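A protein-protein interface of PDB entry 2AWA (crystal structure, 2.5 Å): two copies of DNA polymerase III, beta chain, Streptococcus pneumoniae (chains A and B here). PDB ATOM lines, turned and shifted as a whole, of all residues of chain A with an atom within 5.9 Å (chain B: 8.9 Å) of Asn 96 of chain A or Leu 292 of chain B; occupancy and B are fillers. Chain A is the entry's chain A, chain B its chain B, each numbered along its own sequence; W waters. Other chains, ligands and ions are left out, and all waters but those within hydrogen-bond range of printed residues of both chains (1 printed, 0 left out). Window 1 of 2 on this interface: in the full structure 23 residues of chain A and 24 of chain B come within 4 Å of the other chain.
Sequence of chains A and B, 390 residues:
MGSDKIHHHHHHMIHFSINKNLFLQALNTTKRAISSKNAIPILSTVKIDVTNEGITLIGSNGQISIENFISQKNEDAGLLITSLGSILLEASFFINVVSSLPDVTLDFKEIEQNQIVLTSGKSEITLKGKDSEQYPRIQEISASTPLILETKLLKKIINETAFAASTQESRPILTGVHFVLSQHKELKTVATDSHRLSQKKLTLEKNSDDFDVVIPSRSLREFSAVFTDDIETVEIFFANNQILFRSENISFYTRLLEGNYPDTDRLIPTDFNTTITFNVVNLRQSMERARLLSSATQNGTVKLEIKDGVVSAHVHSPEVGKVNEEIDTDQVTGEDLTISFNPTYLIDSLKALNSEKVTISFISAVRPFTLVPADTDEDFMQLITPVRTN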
ATOM      1  N   LEU A  24     -25.209  12.549  41.668  1.00  0.00           N
ATOM      2  CA  LEU A  24     -25.836  12.871  40.395  1.00  0.00           C
ATOM      3  C   LEU A  24     -27.150  13.599  40.617  1.00  0.00           C
ATOM      4  O   LEU A  24     -27.382  14.642  40.030  1.00  0.00           O
ATOM      5  CB  LEU A  24     -26.055  11.616  39.602  1.00  0.00           C
ATOM      6  CG  LEU A  24     -26.482  11.790  38.150  1.00  0.00           C
ATOM      7  CD1 LEU A  24     -25.559  12.736  37.393  1.00  0.00           C
ATOM      8  CD2 LEU A  24     -26.529  10.416  37.492  1.00  0.00           C
ATOM      9  N   ALA A  91     -20.767  22.313  33.756  1.00  0.00           N
ATOM     10  CA  ALA A  91     -21.846  21.457  34.271  1.00  0.00           C
ATOM     11  C   ALA A  91     -22.351  20.363  33.322  1.00  0.00           C
ATOM     12  O   ALA A  91     -22.309  19.193  33.675  1.00  0.00           O
ATOM     13  CB  ALA A  91     -23.009  22.301  34.750  1.00  0.00           C
ATOM     14  N   SER A  92     -22.841  20.707  32.137  1.00  0.00           N
ATOM     15  CA  SER A  92     -23.461  19.652  31.297  1.00  0.00           C
ATOM     16  C   SER A  92     -22.524  18.491  31.030  1.00  0.00           C
ATOM     17  O   SER A  92     -22.907  17.348  31.211  1.00  0.00           O
ATOM     18  CB  SER A  92     -23.955  20.178  29.969  1.00  0.00           C
ATOM     19  OG  SER A  92     -24.859  21.214  30.207  1.00  0.00           O
ATOM     20  N   PHE A  93     -21.297  18.777  30.615  1.00  0.00           N
ATOM     21  CA  PHE A  93     -20.343  17.722  30.322  1.00  0.00           C
ATOM     22  C   PHE A  93     -20.062  16.879  31.566  1.00  0.00           C
ATOM     23  O   PHE A  93     -20.146  15.682  31.522  1.00  0.00           O
ATOM     24  CB  PHE A  93     -19.048  18.299  29.755  1.00  0.00           C
ATOM     25  CG  PHE A  93     -18.145  17.275  29.199  1.00  0.00           C
ATOM     26  CD1 PHE A  93     -18.519  16.551  28.074  1.00  0.00           C
ATOM     27  CD2 PHE A  93     -16.944  16.975  29.808  1.00  0.00           C
ATOM     28  CE1 PHE A  93     -17.704  15.555  27.566  1.00  0.00           C
ATOM     29  CE2 PHE A  93     -16.115  15.991  29.289  1.00  0.00           C
ATOM     30  CZ  PHE A  93     -16.498  15.287  28.165  1.00  0.00           C
ATOM     31  N   PHE A  94     -19.755  17.519  32.685  1.00  0.00           N
ATOM     32  CA  PHE A  94     -19.400  16.822  33.902  1.00  0.00           C
ATOM     33  C   PHE A  94     -20.520  15.908  34.343  1.00  0.00           C
ATOM     34  O   PHE A  94     -20.314  14.742  34.664  1.00  0.00           O
ATOM     35  CB  PHE A  94     -19.117  17.853  34.986  1.00  0.00           C
ATOM     36  CG  PHE A  94     -18.873  17.272  36.341  1.00  0.00           C
ATOM     37  CD1 PHE A  94     -17.976  16.232  36.524  1.00  0.00           C
ATOM     38  CD2 PHE A  94     -19.522  17.783  37.444  1.00  0.00           C
ATOM     39  CE1 PHE A  94     -17.734  15.740  37.787  1.00  0.00           C
ATOM     40  CE2 PHE A  94     -19.277  17.280  38.706  1.00  0.00           C
ATOM     41  CZ  PHE A  94     -18.397  16.258  38.868  1.00  0.00           C
ATOM     42  N   ILE A  95     -21.720  16.456  34.348  1.00  0.00           N
ATOM     43  CA  ILE A  95     -22.890  15.710  34.735  1.00  0.00           C
ATOM     44  C   ILE A  95     -23.108  14.520  33.847  1.00  0.00           C
ATOM     45  O   ILE A  95     -23.536  13.481  34.328  1.00  0.00           O
ATOM     46  CB  ILE A  95     -24.137  16.576  34.709  1.00  0.00           C
ATOM     47  CG1 ILE A  95     -24.137  17.496  35.925  1.00  0.00           C
ATOM     48  CG2 ILE A  95     -25.379  15.704  34.717  1.00  0.00           C
ATOM     49  CD1 ILE A  95     -25.380  18.383  36.010  1.00  0.00           C
ATOM     50  N   ASN A  96     -22.832  14.662  32.560  1.00  0.00           N
ATOM     51  CA  ASN A  96     -22.904  13.520  31.630  1.00  0.00           C
ATOM     52  C   ASN A  96     -21.861  12.445  31.892  1.00  0.00           C
ATOM     53  O   ASN A  96     -22.129  11.259  31.765  1.00  0.00           O
ATOM     54  CB  ASN A  96     -22.757  14.002  30.198  1.00  0.00           C
ATOM     55  CG  ASN A  96     -24.039  14.551  29.642  1.00  0.00           C
ATOM     56  OD1 ASN A  96     -25.118  14.281  30.171  1.00  0.00           O
ATOM     57  ND2 ASN A  96     -23.943  15.289  28.545  1.00  0.00           N
ATOM     58  N   VAL A  97     -20.673  12.862  32.276  1.00  0.00           N
ATOM     59  CA  VAL A  97     -19.602  11.938  32.571  1.00  0.00           C
ATOM     60  C   VAL A  97     -19.939  11.142  33.839  1.00  0.00           C
ATOM     61  O   VAL A  97     -19.882   9.914  33.832  1.00  0.00           O
ATOM     62  CB  VAL A  97     -18.244  12.696  32.670  1.00  0.00           C
ATOM     63  CG1 VAL A  97     -17.133  11.812  33.265  1.00  0.00           C
ATOM     64  CG2 VAL A  97     -17.851  13.185  31.284  1.00  0.00           C
ATOM     65  N   VAL A  98     -20.321  11.840  34.906  1.00  0.00           N
ATOM     66  CA  VAL A  98     -20.656  11.176  36.155  1.00  0.00           C
ATOM     67  C   VAL A  98     -21.787  10.161  35.912  1.00  0.00           C
ATOM     68  O   VAL A  98     -21.721   8.963  36.243  1.00  0.00           O
ATOM     69  CB  VAL A  98     -21.081  12.205  37.204  1.00  0.00           C
ATOM     70  CG1 VAL A  98     -21.739  11.538  38.402  1.00  0.00           C
ATOM     71  CG2 VAL A  98     -19.886  13.045  37.639  1.00  0.00           C
ATOM     72  N   SER A  99     -22.844  10.660  35.316  1.00  0.00           N
ATOM     73  CA  SER A  99     -23.945   9.795  34.910  1.00  0.00           C
ATOM     74  C   SER A  99     -23.476   8.517  34.183  1.00  0.00           C
ATOM     75  O   SER A  99     -24.079   7.472  34.344  1.00  0.00           O
ATOM     76  CB  SER A  99     -24.904  10.568  34.041  1.00  0.00           C
ATOM     77  OG  SER A  99     -25.955   9.718  33.756  1.00  0.00           O
ATOM     78  N   SER A 100     -22.391   8.578  33.417  1.00  0.00           N
ATOM     79  CA  SER A 100     -21.939   7.409  32.624  1.00  0.00           C
ATOM     80  C   SER A 100     -21.060   6.418  33.375  1.00  0.00           C
ATOM     81  O   SER A 100     -20.769   5.358  32.862  1.00  0.00           O
ATOM     82  CB  SER A 100     -21.140   7.883  31.431  1.00  0.00           C
ATOM     83  OG  SER A 100     -19.896   8.412  31.885  1.00  0.00           O
ATOM     84  N   LEU A 101     -20.623   6.766  34.567  1.00  0.00           N
ATOM     85  CA  LEU A 101     -19.684   5.933  35.315  1.00  0.00           C
ATOM     86  C   LEU A 101     -20.338   4.636  35.807  1.00  0.00           C
ATOM     87  O   LEU A 101     -21.513   4.642  36.190  1.00  0.00           O
ATOM     88  CB  LEU A 101     -19.121   6.730  36.505  1.00  0.00           C
ATOM     89  CG  LEU A 101     -18.253   7.934  36.143  1.00  0.00           C
ATOM     90  CD1 LEU A 101     -17.964   8.811  37.338  1.00  0.00           C
ATOM     91  CD2 LEU A 101     -16.953   7.527  35.514  1.00  0.00           C
ATOM     92  N   GLN B 285     -20.860  -0.078  27.155  1.00  0.00           N
ATOM     93  CA  GLN B 285     -20.805   0.987  28.148  1.00  0.00           C
ATOM     94  C   GLN B 285     -19.411   1.579  28.225  1.00  0.00           C
ATOM     95  O   GLN B 285     -19.264   2.770  28.465  1.00  0.00           O
ATOM     96  CB  GLN B 285     -21.283   0.483  29.497  1.00  0.00           C
ATOM     97  CG  GLN B 285     -22.777   0.113  29.472  1.00  0.00           C
ATOM     98  CD  GLN B 285     -23.230  -0.685  30.673  1.00  0.00           C
ATOM     99  OE1 GLN B 285     -22.427  -1.185  31.454  1.00  0.00           O
ATOM    100  NE2 GLN B 285     -24.534  -0.819  30.816  1.00  0.00           N
ATOM    101  N   SER B 286     -18.393   0.761  27.982  1.00  0.00           N
ATOM    102  CA  SER B 286     -17.014   1.256  27.951  1.00  0.00           C
ATOM    103  C   SER B 286     -16.753   2.173  26.772  1.00  0.00           C
ATOM    104  O   SER B 286     -16.058   3.164  26.906  1.00  0.00           O
ATOM    105  CB  SER B 286     -16.024   0.100  27.900  1.00  0.00           C
ATOM    106  OG  SER B 286     -15.937  -0.510  29.165  1.00  0.00           O
ATOM    107  N   MET B 287     -17.295   1.816  25.609  1.00  0.00           N
ATOM    108  CA  MET B 287     -17.137   2.609  24.402  1.00  0.00           C
ATOM    109  C   MET B 287     -17.883   3.936  24.413  1.00  0.00           C
ATOM    110  O   MET B 287     -17.434   4.908  23.803  1.00  0.00           O
ATOM    111  CB  MET B 287     -17.583   1.780  23.215  1.00  0.00           C
ATOM    112  CG  MET B 287     -16.665   0.629  22.930  1.00  0.00           C
ATOM    113  SD  MET B 287     -14.758   1.174  22.757  1.00  0.00           S
ATOM    114  CE  MET B 287     -14.096   0.775  24.590  1.00  0.00           C
ATOM    115  N   GLU B 288     -19.016   3.975  25.108  1.00  0.00           N
ATOM    116  CA  GLU B 288     -19.807   5.196  25.273  1.00  0.00           C
ATOM    117  C   GLU B 288     -19.140   6.192  26.199  1.00  0.00           C
ATOM    118  O   GLU B 288     -19.257   7.405  25.999  1.00  0.00           O
ATOM    119  CB  GLU B 288     -21.192   4.850  25.794  1.00  0.00           C
ATOM    120  CG  GLU B 288     -21.911   3.892  24.856  1.00  0.00           C
ATOM    121  CD  GLU B 288     -23.398   4.038  24.812  1.00  0.00           C
ATOM    122  OE1 GLU B 288     -23.877   5.185  24.667  1.00  0.00           O
ATOM    123  OE2 GLU B 288     -24.087   2.987  24.869  1.00  0.00           O
ATOM    124  N   ARG B 289     -18.459   5.677  27.214  1.00  0.00           N
ATOM    125  CA  ARG B 289     -17.642   6.496  28.088  1.00  0.00           C
ATOM    126  C   ARG B 289     -16.472   7.064  27.292  1.00  0.00           C
ATOM    127  O   ARG B 289     -16.238   8.274  27.271  1.00  0.00           O
ATOM    128  CB  ARG B 289     -17.139   5.673  29.298  1.00  0.00           C
ATOM    129  CG  ARG B 289     -18.031   5.771  30.552  1.00  0.00           C
ATOM    130  CD  ARG B 289     -17.407   5.090  31.795  1.00  0.00           C
ATOM    131  NE  ARG B 289     -17.151   3.664  31.580  1.00  0.00           N
ATOM    132  CZ  ARG B 289     -18.018   2.681  31.813  1.00  0.00           C
ATOM    133  NH1 ARG B 289     -19.225   2.929  32.270  1.00  0.00           N
ATOM    134  NH2 ARG B 289     -17.674   1.432  31.560  1.00  0.00           N
ATOM    135  N   ALA B 290     -15.742   6.175  26.638  1.00  0.00           N
ATOM    136  CA  ALA B 290     -14.710   6.572  25.696  1.00  0.00           C
ATOM    137  C   ALA B 290     -15.206   7.663  24.746  1.00  0.00           C
ATOM    138  O   ALA B 290     -14.521   8.642  24.513  1.00  0.00           O
ATOM    139  CB  ALA B 290     -14.250   5.373  24.909  1.00  0.00           C
ATOM    140  N   ARG B 291     -16.409   7.508  24.215  1.00  0.00           N
ATOM    141  CA  ARG B 291     -16.922   8.453  23.226  1.00  0.00           C
ATOM    142  C   ARG B 291     -17.219   9.859  23.782  1.00  0.00           C
ATOM    143  O   ARG B 291     -17.067  10.863  23.078  1.00  0.00           O
ATOM    144  CB  ARG B 291     -18.149   7.872  22.524  1.00  0.00           C
ATOM    145  CG  ARG B 291     -18.712   8.796  21.446  1.00  0.00           C
ATOM    146  CD  ARG B 291     -19.721   8.093  20.542  1.00  0.00           C
ATOM    147  NE  ARG B 291     -20.944   7.769  21.259  1.00  0.00           N
ATOM    148  CZ  ARG B 291     -21.980   7.154  20.714  1.00  0.00           C
ATOM    149  NH1 ARG B 291     -21.954   6.785  19.439  1.00  0.00           N
ATOM    150  NH2 ARG B 291     -23.038   6.896  21.460  1.00  0.00           N
ATOM    151  N   LEU B 292     -17.629   9.944  25.038  1.00  0.00           N
ATOM    152  CA  LEU B 292     -17.842  11.254  25.653  1.00  0.00           C
ATOM    153  C   LEU B 292     -16.641  12.146  25.490  1.00  0.00           C
ATOM    154  O   LEU B 292     -16.795  13.346  25.273  1.00  0.00           O
ATOM    155  CB  LEU B 292     -18.140  11.144  27.150  1.00  0.00           C
ATOM    156  CG  LEU B 292     -19.530  10.639  27.440  1.00  0.00           C
ATOM    157  CD1 LEU B 292     -19.676  10.354  28.902  1.00  0.00           C
ATOM    158  CD2 LEU B 292     -20.536  11.648  26.961  1.00  0.00           C
ATOM    159  N   LEU B 293     -15.448  11.576  25.608  1.00  0.00           N
ATOM    160  CA  LEU B 293     -14.258  12.403  25.506  1.00  0.00           C
ATOM    161  C   LEU B 293     -13.700  12.473  24.108  1.00  0.00           C
ATOM    162  O   LEU B 293     -13.146  13.506  23.734  1.00  0.00           O
ATOM    163  CB  LEU B 293     -13.181  11.966  26.497  1.00  0.00           C
ATOM    164  CG  LEU B 293     -13.484  12.512  27.886  1.00  0.00           C
ATOM    165  CD1 LEU B 293     -14.216  11.482  28.710  1.00  0.00           C
ATOM    166  CD2 LEU B 293     -12.221  12.962  28.566  1.00  0.00           C
ATOM    167  N   SER B 294     -13.829  11.396  23.337  1.00  0.00           N
ATOM    168  CA  SER B 294     -13.240  11.373  22.000  1.00  0.00           C
ATOM    169  C   SER B 294     -14.024  12.247  21.034  1.00  0.00           C
ATOM    170  O   SER B 294     -13.459  12.723  20.070  1.00  0.00           O
ATOM    171  CB  SER B 294     -13.093   9.954  21.453  1.00  0.00           C
ATOM    172  OG  SER B 294     -14.346   9.362  21.190  1.00  0.00           O
ATOM    173  N   SER B 295     -15.303  12.491  21.306  1.00  0.00           N
ATOM    174  CA  SER B 295     -16.114  13.333  20.424  1.00  0.00           C
ATOM    175  C   SER B 295     -15.847  14.822  20.598  1.00  0.00           C
ATOM    176  O   SER B 295     -16.286  15.617  19.771  1.00  0.00           O
ATOM    177  CB  SER B 295     -17.604  13.041  20.584  1.00  0.00           C
ATOM    178  OG  SER B 295     -17.979  13.007  21.940  1.00  0.00           O
ATOM    179  N   ALA B 296     -15.125  15.210  21.647  1.00  0.00           N
ATOM    180  CA  ALA B 296     -14.589  16.575  21.725  1.00  0.00           C
ATOM    181  C   ALA B 296     -13.512  16.847  20.648  1.00  0.00           C
ATOM    182  O   ALA B 296     -13.300  17.995  20.261  1.00  0.00           O
ATOM    183  CB  ALA B 296     -14.046  16.859  23.132  1.00  0.00           C
ATOM    184  N   THR B 297     -12.839  15.795  20.173  1.00  0.00           N
ATOM    185  CA  THR B 297     -11.860  15.892  19.070  1.00  0.00           C
ATOM    186  C   THR B 297     -12.558  15.654  17.729  1.00  0.00           C
ATOM    187  O   THR B 297     -13.613  15.006  17.690  1.00  0.00           O
ATOM    188  CB  THR B 297     -10.744  14.790  19.169  1.00  0.00           C
ATOM    189  OG1 THR B 297     -10.516  14.395  20.538  1.00  0.00           O
ATOM    190  CG2 THR B 297      -9.437  15.264  18.494  1.00  0.00           C
ATOM    191  N   VAL B 302     -10.899   6.120  19.907  1.00  0.00           N
ATOM    192  CA  VAL B 302     -10.561   5.394  21.118  1.00  0.00           C
ATOM    193  C   VAL B 302      -9.402   4.475  20.726  1.00  0.00           C
ATOM    194  O   VAL B 302      -9.315   4.028  19.591  1.00  0.00           O
ATOM    195  CB  VAL B 302     -11.794   4.569  21.647  1.00  0.00           C
ATOM    196  CG1 VAL B 302     -12.118   3.384  20.729  1.00  0.00           C
ATOM    197  CG2 VAL B 302     -11.573   4.071  23.058  1.00  0.00           C
ATOM    198  N   VAL B 315      -8.424   7.464  25.749  1.00  0.00           N
ATOM    199  CA  VAL B 315      -8.767   8.628  24.968  1.00  0.00           C
ATOM    200  C   VAL B 315      -8.029   9.790  25.586  1.00  0.00           C
ATOM    201  O   VAL B 315      -8.035   9.954  26.801  1.00  0.00           O
ATOM    202  CB  VAL B 315     -10.286   8.934  25.021  1.00  0.00           C
ATOM    203  CG1 VAL B 315     -10.605  10.224  24.248  1.00  0.00           C
ATOM    204  CG2 VAL B 315     -11.119   7.736  24.476  1.00  0.00           C
ATOM    205  N   SER B 317      -8.194  13.799  25.073  1.00  0.00           N
ATOM    206  CA  SER B 317      -8.746  14.994  24.451  1.00  0.00           C
ATOM    207  C   SER B 317      -8.131  16.238  25.083  1.00  0.00           C
ATOM    208  O   SER B 317      -8.561  16.674  26.137  1.00  0.00           O
ATOM    209  CB  SER B 317     -10.258  14.992  24.598  1.00  0.00           C
ATOM    210  OG  SER B 317     -10.791  16.091  23.911  1.00  0.00           O
ATOM    211  N   VAL B 320      -9.670  19.095  27.436  1.00  0.00           N
ATOM    212  CA  VAL B 320     -10.930  18.580  27.975  1.00  0.00           C
ATOM    213  C   VAL B 320     -10.769  17.435  28.967  1.00  0.00           C
ATOM    214  O   VAL B 320     -11.345  17.491  30.047  1.00  0.00           O
ATOM    215  CB  VAL B 320     -11.883  18.113  26.855  1.00  0.00           C
ATOM    216  CG1 VAL B 320     -13.288  17.784  27.448  1.00  0.00           C
ATOM    217  CG2 VAL B 320     -11.958  19.212  25.745  1.00  0.00           C
ATOM    218  N   GLY B 321     -10.027  16.389  28.603  1.00  0.00           N
ATOM    219  CA  GLY B 321      -9.758  15.314  29.550  1.00  0.00           C
ATOM    220  C   GLY B 321      -9.201  14.041  28.963  1.00  0.00           C
ATOM    221  O   GLY B 321      -8.707  14.017  27.855  1.00  0.00           O
ATOM    222  N   LYS B 322      -9.316  12.959  29.709  1.00  0.00           N
ATOM    223  CA  LYS B 322      -8.587  11.753  29.396  1.00  0.00           C
ATOM    224  C   LYS B 322      -9.342  10.573  30.027  1.00  0.00           C
ATOM    225  O   LYS B 322      -9.902  10.708  31.113  1.00  0.00           O
ATOM    226  CB  LYS B 322      -7.137  11.947  29.893  1.00  0.00           C
ATOM    227  CG  LYS B 322      -6.296  10.718  30.150  1.00  0.00           C
ATOM    228  CD  LYS B 322      -4.943  11.120  30.810  1.00  0.00           C
ATOM    229  CE  LYS B 322      -3.936   9.935  30.922  1.00  0.00           C
ATOM    230  NZ  LYS B 322      -4.493   8.717  31.631  1.00  0.00           N
ATOM    231  N   VAL B 323      -9.448   9.476  29.295  1.00  0.00           N
ATOM    232  CA  VAL B 323     -10.113   8.261  29.760  1.00  0.00           C
ATOM    233  C   VAL B 323      -9.079   7.164  29.767  1.00  0.00           C
ATOM    234  O   VAL B 323      -8.419   6.964  28.757  1.00  0.00           O
ATOM    235  CB  VAL B 323     -11.216   7.761  28.789  1.00  0.00           C
ATOM    236  CG1 VAL B 323     -11.909   6.542  29.351  1.00  0.00           C
ATOM    237  CG2 VAL B 323     -12.235   8.816  28.524  1.00  0.00           C
ATOM    238  N   PRO B 343     -15.208   4.989  17.966  1.00  0.00           N
ATOM    239  CA  PRO B 343     -16.000   4.207  18.899  1.00  0.00           C
ATOM    240  C   PRO B 343     -17.486   4.121  18.522  1.00  0.00           C
ATOM    241  O   PRO B 343     -18.169   3.189  18.965  1.00  0.00           O
ATOM    242  CB  PRO B 343     -15.812   4.949  20.220  1.00  0.00           C
ATOM    243  CG  PRO B 343     -15.536   6.364  19.831  1.00  0.00           C
ATOM    244  CD  PRO B 343     -14.726   6.250  18.568  1.00  0.00           C
ATOM    245  N   THR B 344     -17.978   5.044  17.699  1.00  0.00           N
ATOM    246  CA  THR B 344     -19.384   5.031  17.317  1.00  0.00           C
ATOM    247  C   THR B 344     -19.656   3.774  16.501  1.00  0.00           C
ATOM    248  O   THR B 344     -20.682   3.134  16.697  1.00  0.00           O
ATOM    249  CB  THR B 344     -19.792   6.293  16.538  1.00  0.00           C
ATOM    250  OG1 THR B 344     -19.623   7.456  17.361  1.00  0.00           O
ATOM    251  CG2 THR B 344     -21.219   6.233  16.101  1.00  0.00           C
ATOM    252  N   ILE B 347     -19.881   0.766  18.826  1.00  0.00           N
ATOM    253  CA  ILE B 347     -21.171   0.859  19.498  1.00  0.00           C
ATOM    254  C   ILE B 347     -22.333   0.416  18.584  1.00  0.00           C
ATOM    255  O   ILE B 347     -23.209  -0.314  19.017  1.00  0.00           O
ATOM    256  CB  ILE B 347     -21.420   2.292  20.009  1.00  0.00           C
ATOM    257  CG1 ILE B 347     -20.494   2.606  21.192  1.00  0.00           C
ATOM    258  CG2 ILE B 347     -22.848   2.458  20.463  1.00  0.00           C
ATOM    259  CD1 ILE B 347     -20.256   4.097  21.416  1.00  0.00           C
HETATM  260  O   HOH W   1     -21.997   4.138  30.054  1.00  0.00           O
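Of the 23 printed residues of chain B, 3 touch a printed residue of chain A.
Printed residues of chain B that touch a printed residue of chain A: Arg 289, Leu 292 and Val 320.
Hydrophobic or aromatic side chains of chain B that line the printed part of chain A: Leu 292 and Val 320.
Of the 12 printed residues of chain A, 4 touch a printed residue of chain B.
Among the printed residues, no Asp or Glu carboxylate lies within 4 Å of a Lys or Arg side-chain nitrogen of the other chain.
The backbone carbonyl oxygen (O) of Ser 100 of chain A lies within hydrogen-bond range of the guanidinium group (NH1) of Arg 289 of chain B, 2.9 Å away.
Water W1 lies within hydrogen-bond range of O of Ser 100 of chain A (3.3 Å) and O of Gln 285 of chain B (3.4 Å).
Among the printed residues, merely in contact across the chains: Phe 93 of chain A with Leu 292 of chain B (3.3 Å), Ser 100 of chain A with Leu 292 of chain B (3.6 Å), Phe 93 of chain A with Val 320 of chain B (3.8 Å), Asn 96 of chain A with Leu 292 of chain B (3.9 Å) and Val 97 of chain A with Leu 292 of chain B (3.997 Å).
No position is printed for both chains.
The side-chain hydroxyl (OG) of Ser 100 of chain A sits at hydrogen-bond distance from the backbone carbonyl oxygen (O) of Val 97 of chain A (2.5 Å).
Of the printed residues of chain B, Phe 93 of chain A touches Leu 292 and Val 320.
Of chain B, only Leu 292 comes within 4 Å of Asn 96 of chain A.
Val 98 of chain A touches none of the printed residues of chain B.
Of the printed residues of chain B, Ser 100 of chain A touches Arg 289 and Leu 292.
Of the printed residues of chain A, Leu 292 of chain B touches Phe 93 (3.3 Å), Asn 96 (3.9 Å), Val 97 (3.997 Å) and Ser 100 (3.6 Å).
The nearest printed residue of chain A that does not touch Leu 292 of chain B is Val 98 of chain A (6.2 Å).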
